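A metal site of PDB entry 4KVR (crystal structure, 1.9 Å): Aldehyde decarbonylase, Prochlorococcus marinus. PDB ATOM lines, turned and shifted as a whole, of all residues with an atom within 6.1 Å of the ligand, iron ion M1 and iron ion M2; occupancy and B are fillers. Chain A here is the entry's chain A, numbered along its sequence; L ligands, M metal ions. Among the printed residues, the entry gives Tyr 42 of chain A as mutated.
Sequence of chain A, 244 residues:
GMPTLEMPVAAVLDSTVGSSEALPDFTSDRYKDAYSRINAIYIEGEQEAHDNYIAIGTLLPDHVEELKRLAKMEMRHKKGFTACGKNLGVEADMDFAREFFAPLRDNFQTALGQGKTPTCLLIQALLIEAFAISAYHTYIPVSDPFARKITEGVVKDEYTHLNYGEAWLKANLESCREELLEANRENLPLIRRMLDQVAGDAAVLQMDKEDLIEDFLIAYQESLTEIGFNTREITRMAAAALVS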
ATOM      1  N   ILE A  41     -12.863 -21.963 -29.751  1.00  0.00           N
ATOM      2  CA  ILE A  41     -11.711 -21.418 -29.032  1.00  0.00           C
ATOM      3  C   ILE A  41     -11.922 -19.924 -28.726  1.00  0.00           C
ATOM      4  O   ILE A  41     -11.685 -19.490 -27.595  1.00  0.00           O
ATOM      5  CB  ILE A  41     -10.410 -21.720 -29.775  1.00  0.00           C
ATOM      6  CG1 ILE A  41     -10.067 -23.204 -29.611  1.00  0.00           C
ATOM      7  CG2 ILE A  41      -9.261 -20.814 -29.256  1.00  0.00           C
ATOM      8  CD1 ILE A  41      -9.002 -23.696 -30.580  1.00  0.00           C
ATOM      9  N   TYR A  42     -12.396 -19.159 -29.712  1.00  0.00           N
ATOM     10  CA  TYR A  42     -12.716 -17.755 -29.483  1.00  0.00           C
ATOM     11  C   TYR A  42     -13.705 -17.614 -28.317  1.00  0.00           C
ATOM     12  O   TYR A  42     -13.464 -16.885 -27.361  1.00  0.00           O
ATOM     13  CB  TYR A  42     -13.329 -17.122 -30.728  1.00  0.00           C
ATOM     14  CG  TYR A  42     -12.437 -17.054 -31.958  1.00  0.00           C
ATOM     15  CD1 TYR A  42     -11.070 -17.305 -31.885  1.00  0.00           C
ATOM     16  CD2 TYR A  42     -12.978 -16.725 -33.188  1.00  0.00           C
ATOM     17  CE1 TYR A  42     -10.276 -17.230 -33.022  1.00  0.00           C
ATOM     18  CE2 TYR A  42     -12.200 -16.648 -34.321  1.00  0.00           C
ATOM     19  CZ  TYR A  42     -10.855 -16.903 -34.239  1.00  0.00           C
ATOM     20  OH  TYR A  42     -10.111 -16.814 -35.394  1.00  0.00           O
ATOM     21  N   ILE A  43     -14.827 -18.329 -28.415  1.00  0.00           N
ATOM     22  CA  ILE A  43     -15.871 -18.257 -27.396  1.00  0.00           C
ATOM     23  C   ILE A  43     -15.361 -18.633 -26.007  1.00  0.00           C
ATOM     24  O   ILE A  43     -15.551 -17.881 -25.038  1.00  0.00           O
ATOM     25  CB  ILE A  43     -17.073 -19.128 -27.776  1.00  0.00           C
ATOM     26  CG1 ILE A  43     -17.743 -18.543 -29.028  1.00  0.00           C
ATOM     27  CG2 ILE A  43     -18.066 -19.187 -26.628  1.00  0.00           C
ATOM     28  CD1 ILE A  43     -18.739 -19.506 -29.680  1.00  0.00           C
ATOM     29  N   GLU A  44     -14.682 -19.768 -25.908  1.00  0.00           N
ATOM     30  CA  GLU A  44     -14.163 -20.215 -24.617  1.00  0.00           C
ATOM     31  C   GLU A  44     -13.119 -19.244 -24.076  1.00  0.00           C
ATOM     32  O   GLU A  44     -13.042 -19.008 -22.864  1.00  0.00           O
ATOM     33  CB  GLU A  44     -13.581 -21.625 -24.715  1.00  0.00           C
ATOM     34  CG  GLU A  44     -12.997 -22.183 -23.410  1.00  0.00           C
ATOM     35  CD  GLU A  44     -14.035 -22.399 -22.330  1.00  0.00           C
ATOM     36  OE1 GLU A  44     -15.249 -22.446 -22.640  1.00  0.00           O
ATOM     37  OE2 GLU A  44     -13.664 -22.515 -21.145  1.00  0.00           O
ATOM     38  N   GLY A  45     -12.313 -18.688 -24.975  1.00  0.00           N
ATOM     39  CA  GLY A  45     -11.263 -17.759 -24.596  1.00  0.00           C
ATOM     40  C   GLY A  45     -11.861 -16.511 -23.958  1.00  0.00           C
ATOM     41  O   GLY A  45     -11.380 -16.041 -22.937  1.00  0.00           O
ATOM     42  N   GLU A  46     -12.915 -15.999 -24.565  1.00  0.00           N
ATOM     43  CA  GLU A  46     -13.604 -14.822 -24.019  1.00  0.00           C
ATOM     44  C   GLU A  46     -14.218 -15.149 -22.661  1.00  0.00           C
ATOM     45  O   GLU A  46     -14.100 -14.372 -21.725  1.00  0.00           O
ATOM     46  CB  GLU A  46     -14.687 -14.323 -24.983  1.00  0.00           C
ATOM     47  CG  GLU A  46     -14.207 -13.953 -26.381  1.00  0.00           C
ATOM     48  CD  GLU A  46     -13.175 -12.844 -26.383  1.00  0.00           C
ATOM     49  OE1 GLU A  46     -13.083 -12.100 -25.380  1.00  0.00           O
ATOM     50  OE2 GLU A  46     -12.476 -12.699 -27.404  1.00  0.00           O
ATOM     51  N   ALA A  49     -11.453 -15.377 -20.023  1.00  0.00           N
ATOM     52  CA  ALA A  49     -10.968 -14.024 -19.772  1.00  0.00           C
ATOM     53  C   ALA A  49     -11.887 -13.312 -18.775  1.00  0.00           C
ATOM     54  O   ALA A  49     -11.422 -12.732 -17.791  1.00  0.00           O
ATOM     55  CB  ALA A  49     -10.857 -13.250 -21.082  1.00  0.00           C
ATOM     56  N   TYR A  53     -10.519 -12.128 -15.044  1.00  0.00           N
ATOM     57  CA  TYR A  53     -10.565 -10.770 -14.526  1.00  0.00           C
ATOM     58  C   TYR A  53     -11.366 -10.667 -13.216  1.00  0.00           C
ATOM     59  O   TYR A  53     -10.946  -9.971 -12.296  1.00  0.00           O
ATOM     60  CB  TYR A  53     -11.058  -9.792 -15.602  1.00  0.00           C
ATOM     61  CG  TYR A  53     -10.022  -9.555 -16.675  1.00  0.00           C
ATOM     62  CD1 TYR A  53      -8.739  -9.154 -16.319  1.00  0.00           C
ATOM     63  CD2 TYR A  53     -10.301  -9.780 -18.023  1.00  0.00           C
ATOM     64  CE1 TYR A  53      -7.766  -8.945 -17.284  1.00  0.00           C
ATOM     65  CE2 TYR A  53      -9.320  -9.586 -18.998  1.00  0.00           C
ATOM     66  CZ  TYR A  53      -8.051  -9.162 -18.608  1.00  0.00           C
ATOM     67  OH  TYR A  53      -7.058  -8.956 -19.536  1.00  0.00           O
ATOM     68  N   MET A  73     -16.672  -6.549 -20.835  1.00  0.00           N
ATOM     69  CA  MET A  73     -16.279  -6.445 -22.230  1.00  0.00           C
ATOM     70  C   MET A  73     -16.059  -7.844 -22.797  1.00  0.00           C
ATOM     71  O   MET A  73     -16.443  -8.120 -23.918  1.00  0.00           O
ATOM     72  CB  MET A  73     -14.971  -5.654 -22.413  1.00  0.00           C
ATOM     73  CG  MET A  73     -14.941  -4.258 -21.822  1.00  0.00           C
ATOM     74  SD  MET A  73     -13.318  -3.471 -22.065  1.00  0.00           S
ATOM     75  CE  MET A  73     -13.057  -3.908 -23.770  1.00  0.00           C
ATOM     76  N   GLU A  74     -15.432  -8.709 -21.997  1.00  0.00           N
ATOM     77  CA  GLU A  74     -15.164 -10.066 -22.459  1.00  0.00           C
ATOM     78  C   GLU A  74     -16.459 -10.802 -22.758  1.00  0.00           C
ATOM     79  O   GLU A  74     -16.526 -11.616 -23.681  1.00  0.00           O
ATOM     80  CB  GLU A  74     -14.336 -10.850 -21.431  1.00  0.00           C
ATOM     81  CG  GLU A  74     -12.980 -10.210 -21.066  1.00  0.00           C
ATOM     82  CD  GLU A  74     -11.960 -10.184 -22.205  1.00  0.00           C
ATOM     83  OE1 GLU A  74     -12.322 -10.305 -23.382  1.00  0.00           O
ATOM     84  OE2 GLU A  74     -10.750 -10.028 -21.902  1.00  0.00           O
ATOM     85  N   HIS A  77     -17.646  -9.717 -26.069  1.00  0.00           N
ATOM     86  CA  HIS A  77     -16.853 -10.395 -27.087  1.00  0.00           C
ATOM     87  C   HIS A  77     -17.399 -11.818 -27.298  1.00  0.00           C
ATOM     88  O   HIS A  77     -17.512 -12.278 -28.421  1.00  0.00           O
ATOM     89  CB  HIS A  77     -15.382 -10.481 -26.636  1.00  0.00           C
ATOM     90  CG  HIS A  77     -14.684  -9.158 -26.533  1.00  0.00           C
ATOM     91  ND1 HIS A  77     -13.444  -9.011 -25.936  1.00  0.00           N
ATOM     92  CD2 HIS A  77     -15.032  -7.926 -26.976  1.00  0.00           C
ATOM     93  CE1 HIS A  77     -13.079  -7.743 -26.002  1.00  0.00           C
ATOM     94  NE2 HIS A  77     -14.018  -7.069 -26.630  1.00  0.00           N
ATOM     95  N   PHE A 101      -7.697 -25.022 -23.682  1.00  0.00           N
ATOM     96  CA  PHE A 101      -7.328 -24.026 -22.682  1.00  0.00           C
ATOM     97  C   PHE A 101      -6.925 -24.643 -21.340  1.00  0.00           C
ATOM     98  O   PHE A 101      -6.442 -23.942 -20.459  1.00  0.00           O
ATOM     99  CB  PHE A 101      -8.450 -23.008 -22.467  1.00  0.00           C
ATOM    100  CG  PHE A 101      -8.494 -21.921 -23.506  1.00  0.00           C
ATOM    101  CD1 PHE A 101      -7.533 -20.922 -23.511  1.00  0.00           C
ATOM    102  CD2 PHE A 101      -9.453 -21.926 -24.489  1.00  0.00           C
ATOM    103  CE1 PHE A 101      -7.558 -19.925 -24.483  1.00  0.00           C
ATOM    104  CE2 PHE A 101      -9.479 -20.921 -25.473  1.00  0.00           C
ATOM    105  CZ  PHE A 101      -8.533 -19.927 -25.462  1.00  0.00           C
ATOM    106  N   GLN A 124      -3.067 -14.003 -18.015  1.00  0.00           N
ATOM    107  CA  GLN A 124      -4.296 -13.464 -18.649  1.00  0.00           C
ATOM    108  C   GLN A 124      -4.085 -12.169 -19.437  1.00  0.00           C
ATOM    109  O   GLN A 124      -4.360 -12.117 -20.633  1.00  0.00           O
ATOM    110  CB  GLN A 124      -5.422 -13.244 -17.634  1.00  0.00           C
ATOM    111  CG  GLN A 124      -6.650 -12.519 -18.251  1.00  0.00           C
ATOM    112  CD  GLN A 124      -7.272 -13.288 -19.410  1.00  0.00           C
ATOM    113  OE1 GLN A 124      -7.495 -14.500 -19.310  1.00  0.00           O
ATOM    114  NE2 GLN A 124      -7.551 -12.593 -20.517  1.00  0.00           N
ATOM    115  N   ILE A 128      -2.514 -14.441 -22.814  1.00  0.00           N
ATOM    116  CA  ILE A 128      -3.805 -14.715 -23.452  1.00  0.00           C
ATOM    117  C   ILE A 128      -4.307 -13.532 -24.302  1.00  0.00           C
ATOM    118  O   ILE A 128      -4.819 -13.747 -25.393  1.00  0.00           O
ATOM    119  CB  ILE A 128      -4.847 -15.180 -22.413  1.00  0.00           C
ATOM    120  CG1 ILE A 128      -4.544 -16.619 -22.004  1.00  0.00           C
ATOM    121  CG2 ILE A 128      -6.245 -15.145 -22.983  1.00  0.00           C
ATOM    122  CD1 ILE A 128      -5.313 -17.070 -20.798  1.00  0.00           C
ATOM    123  N   GLU A 129      -4.135 -12.306 -23.821  1.00  0.00           N
ATOM    124  CA  GLU A 129      -4.521 -11.156 -24.640  1.00  0.00           C
ATOM    125  C   GLU A 129      -3.674 -11.059 -25.905  1.00  0.00           C
ATOM    126  O   GLU A 129      -4.209 -10.777 -26.971  1.00  0.00           O
ATOM    127  CB  GLU A 129      -4.454  -9.833 -23.864  1.00  0.00           C
ATOM    128  CG  GLU A 129      -5.351  -9.785 -22.653  1.00  0.00           C
ATOM    129  CD  GLU A 129      -6.855  -9.710 -22.980  1.00  0.00           C
ATOM    130  OE1 GLU A 129      -7.248  -9.483 -24.151  1.00  0.00           O
ATOM    131  OE2 GLU A 129      -7.652  -9.839 -22.029  1.00  0.00           O
ATOM    132  N   PHE A 131      -2.284 -13.573 -27.413  1.00  0.00           N
ATOM    133  CA  PHE A 131      -2.690 -14.694 -28.260  1.00  0.00           C
ATOM    134  C   PHE A 131      -3.969 -14.289 -28.998  1.00  0.00           C
ATOM    135  O   PHE A 131      -4.132 -14.562 -30.197  1.00  0.00           O
ATOM    136  CB  PHE A 131      -2.925 -15.929 -27.406  1.00  0.00           C
ATOM    137  CG  PHE A 131      -3.396 -17.120 -28.179  1.00  0.00           C
ATOM    138  CD1 PHE A 131      -2.493 -17.890 -28.916  1.00  0.00           C
ATOM    139  CD2 PHE A 131      -4.738 -17.474 -28.194  1.00  0.00           C
ATOM    140  CE1 PHE A 131      -2.936 -18.993 -29.645  1.00  0.00           C
ATOM    141  CE2 PHE A 131      -5.192 -18.568 -28.925  1.00  0.00           C
ATOM    142  CZ  PHE A 131      -4.285 -19.332 -29.650  1.00  0.00           C
ATOM    143  N   ALA A 132      -4.846 -13.623 -28.264  1.00  0.00           N
ATOM    144  CA  ALA A 132      -6.129 -13.170 -28.810  1.00  0.00           C
ATOM    145  C   ALA A 132      -5.921 -12.156 -29.929  1.00  0.00           C
ATOM    146  O   ALA A 132      -6.459 -12.302 -31.023  1.00  0.00           O
ATOM    147  CB  ALA A 132      -6.984 -12.570 -27.724  1.00  0.00           C
ATOM    148  N   ALA A 135      -4.547 -13.829 -33.042  1.00  0.00           N
ATOM    149  CA  ALA A 135      -5.570 -14.623 -33.709  1.00  0.00           C
ATOM    150  C   ALA A 135      -6.550 -13.720 -34.430  1.00  0.00           C
ATOM    151  O   ALA A 135      -6.877 -13.933 -35.603  1.00  0.00           O
ATOM    152  CB  ALA A 135      -6.305 -15.470 -32.701  1.00  0.00           C
ATOM    153  N   TYR A 136      -7.034 -12.705 -33.719  1.00  0.00           N
ATOM    154  CA  TYR A 136      -8.071 -11.825 -34.278  1.00  0.00           C
ATOM    155  C   TYR A 136      -7.529 -10.954 -35.414  1.00  0.00           C
ATOM    156  O   TYR A 136      -8.161 -10.836 -36.462  1.00  0.00           O
ATOM    157  CB  TYR A 136      -8.727 -10.997 -33.175  1.00  0.00           C
ATOM    158  CG  TYR A 136      -9.478 -11.842 -32.163  1.00  0.00           C
ATOM    159  CD1 TYR A 136     -10.086 -13.017 -32.546  1.00  0.00           C
ATOM    160  CD2 TYR A 136      -9.574 -11.460 -30.827  1.00  0.00           C
ATOM    161  CE1 TYR A 136     -10.765 -13.800 -31.647  1.00  0.00           C
ATOM    162  CE2 TYR A 136     -10.266 -12.255 -29.901  1.00  0.00           C
ATOM    163  CZ  TYR A 136     -10.854 -13.426 -30.334  1.00  0.00           C
ATOM    164  OH  TYR A 136     -11.563 -14.239 -29.468  1.00  0.00           O
ATOM    165  N   VAL A 154     -13.583  -6.082 -31.746  1.00  0.00           N
ATOM    166  CA  VAL A 154     -12.915  -6.785 -30.662  1.00  0.00           C
ATOM    167  C   VAL A 154     -11.434  -6.419 -30.514  1.00  0.00           C
ATOM    168  O   VAL A 154     -10.966  -6.176 -29.400  1.00  0.00           O
ATOM    169  CB  VAL A 154     -13.082  -8.317 -30.816  1.00  0.00           C
ATOM    170  CG1 VAL A 154     -12.189  -9.060 -29.821  1.00  0.00           C
ATOM    171  CG2 VAL A 154     -14.545  -8.720 -30.618  1.00  0.00           C
ATOM    172  N   ASP A 157     -10.352  -3.492 -28.528  1.00  0.00           N
ATOM    173  CA  ASP A 157     -10.556  -3.696 -27.104  1.00  0.00           C
ATOM    174  C   ASP A 157      -9.422  -4.422 -26.400  1.00  0.00           C
ATOM    175  O   ASP A 157      -9.109  -4.150 -25.246  1.00  0.00           O
ATOM    176  CB  ASP A 157     -11.832  -4.486 -26.883  1.00  0.00           C
ATOM    177  CG  ASP A 157     -13.072  -3.665 -27.140  1.00  0.00           C
ATOM    178  OD1 ASP A 157     -12.987  -2.428 -26.996  1.00  0.00           O
ATOM    179  OD2 ASP A 157     -14.106  -4.254 -27.490  1.00  0.00           O
ATOM    180  N   GLU A 158      -8.819  -5.405 -27.056  1.00  0.00           N
ATOM    181  CA  GLU A 158      -7.890  -6.230 -26.295  1.00  0.00           C
ATOM    182  C   GLU A 158      -6.576  -5.482 -25.999  1.00  0.00           C
ATOM    183  O   GLU A 158      -5.851  -5.834 -25.079  1.00  0.00           O
ATOM    184  CB  GLU A 158      -7.720  -7.641 -26.914  1.00  0.00           C
ATOM    185  CG  GLU A 158      -9.039  -8.270 -27.495  1.00  0.00           C
ATOM    186  CD  GLU A 158      -9.977  -9.043 -26.506  1.00  0.00           C
ATOM    187  OE1 GLU A 158     -10.020  -8.804 -25.268  1.00  0.00           O
ATOM    188  OE2 GLU A 158     -10.745  -9.914 -27.002  1.00  0.00           O
ATOM    189  N   HIS A 161      -6.911  -4.227 -22.649  1.00  0.00           N
ATOM    190  CA  HIS A 161      -6.633  -5.263 -21.692  1.00  0.00           C
ATOM    191  C   HIS A 161      -5.117  -5.424 -21.497  1.00  0.00           C
ATOM    192  O   HIS A 161      -4.656  -5.539 -20.365  1.00  0.00           O
ATOM    193  CB  HIS A 161      -7.291  -6.566 -22.132  1.00  0.00           C
ATOM    194  CG  HIS A 161      -8.777  -6.460 -22.266  1.00  0.00           C
ATOM    195  ND1 HIS A 161      -9.565  -7.530 -22.642  1.00  0.00           N
ATOM    196  CD2 HIS A 161      -9.615  -5.413 -22.087  1.00  0.00           C
ATOM    197  CE1 HIS A 161     -10.828  -7.144 -22.685  1.00  0.00           C
ATOM    198  NE2 HIS A 161     -10.891  -5.859 -22.355  1.00  0.00           N
HETATM  199  C1  LIG L   1      -9.018 -14.072 -24.625  1.00  0.00           C
HETATM  200  C2  LIG L   1      -9.345 -12.638 -24.368  1.00  0.00           C
HETATM  201  O1  LIG L   1     -10.287 -12.115 -24.990  1.00  0.00           O
HETATM  202  C3  LIG L   1      -9.463 -14.507 -25.992  1.00  0.00           C
HETATM  203  C4  LIG L   1      -8.544 -15.591 -26.475  1.00  0.00           C
HETATM  204  C5  LIG L   1      -9.226 -16.417 -27.519  1.00  0.00           C
HETATM  205  C6  LIG L   1      -8.337 -16.606 -28.702  1.00  0.00           C
HETATM  206  O2  LIG L   1      -8.681 -11.950 -23.552  1.00  0.00           O
HETATM  207 FE    FE M   1     -11.873 -10.461 -25.287  1.00  0.00          FE
HETATM  208 FE    FE M   2      -9.376  -9.587 -23.337  1.00  0.00          FE
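The side-chain hydroxyl (OH) of Tyr 136 is in hydrogen-bond range of the side-chain carboxylate (OE2) of Glu 46 (2.7 Å).
The backbone carbonyl oxygen (O) of Gln 124 is in hydrogen-bond range of the backbone NH (N) of Glu 129 (3.2 Å).
The side-chain carboxylate of Glu 129 lies close to the side-chain hydroxyl of Tyr 53 (2.7 Å).
The side-chain sulfur (SD) of Met 73 lies close to a ring nitrogen (NE2) of His 161, at 3.4 Å.
A ring nitrogen (NE2) of His 77 is in hydrogen-bond range of the side-chain carboxylate (OD2) of Asp 157, 2.9 Å away.
Iron ion M2 is bound by the side-chain carboxylate (OE2) of Glu 74 (2.0 Å), the side-chain carboxylate (OE2) of Glu 129 (2.2 Å), a ring nitrogen (ND1) of His 161 (2.2 Å), the side-chain carboxylate (OE1) of Glu 158 (2.2 Å), the side-chain carboxylate (OE1) of Glu 129 (2.3 Å) and an oxygen (O2) of the ligand (2.5 Å).
Within 4 Å of iron ion M1: Glu 46, Glu 74, His 77 and Glu 158.
The nearest printed residue that does not touch iron ion M1 is His 161 (4.3 Å).
An oxygen (O2) of the ligand sits close to the side-chain amide nitrogen (NE2) of Gln 124, 3.3 Å away.
Of the 23 residues printed, 4 come within 4 Å of iron ion M2.
Along chain A the residues within 4 Å of iron ion M2 span positions 74 to 161.
The nearest printed residue that does not touch iron ion M2 is Tyr 53 (4.3 Å).
Ile 41 touches the ligand.
Gly 45 touches the ligand.
Ala 49 touches the ligand (CB to O2, 3.5 Å).
Ile 128 touches the ligand (CG2 to C1, 3.4 Å).
CE2 of Phe 131 touches C6 of the ligand (3.7 Å).
Ala 132 touches the ligand.
Tyr 136 touches the ligand.
Hydrophobic or aromatic side chains within 4 Å of the ligand: Ala 49, Ile 128, Phe 131 and Ala 132.
Within 4 Å of the ligand: Ile 41, Gly 45, Glu 46, Ala 49, Glu 74, Gln 124, Ile 128, Glu 129, Phe 131, Ala 132, Tyr 136 and Glu 158.
Iron ion M1 is bound by the side-chain carboxylate (OE1) of Glu 74 (2.0 Å), the side-chain carboxylate (OE1) of Glu 46 (2.0 Å), the side-chain carboxylate (OE2) of Glu 158 (2.1 Å), a ring nitrogen (ND1) of His 77 (2.2 Å), an oxygen (O1) of the ligand (2.3 Å) and the side-chain carboxylate (OE1) of Glu 158 (2.5 Å).
Iron ion M1 has six donor atoms within binding distance.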
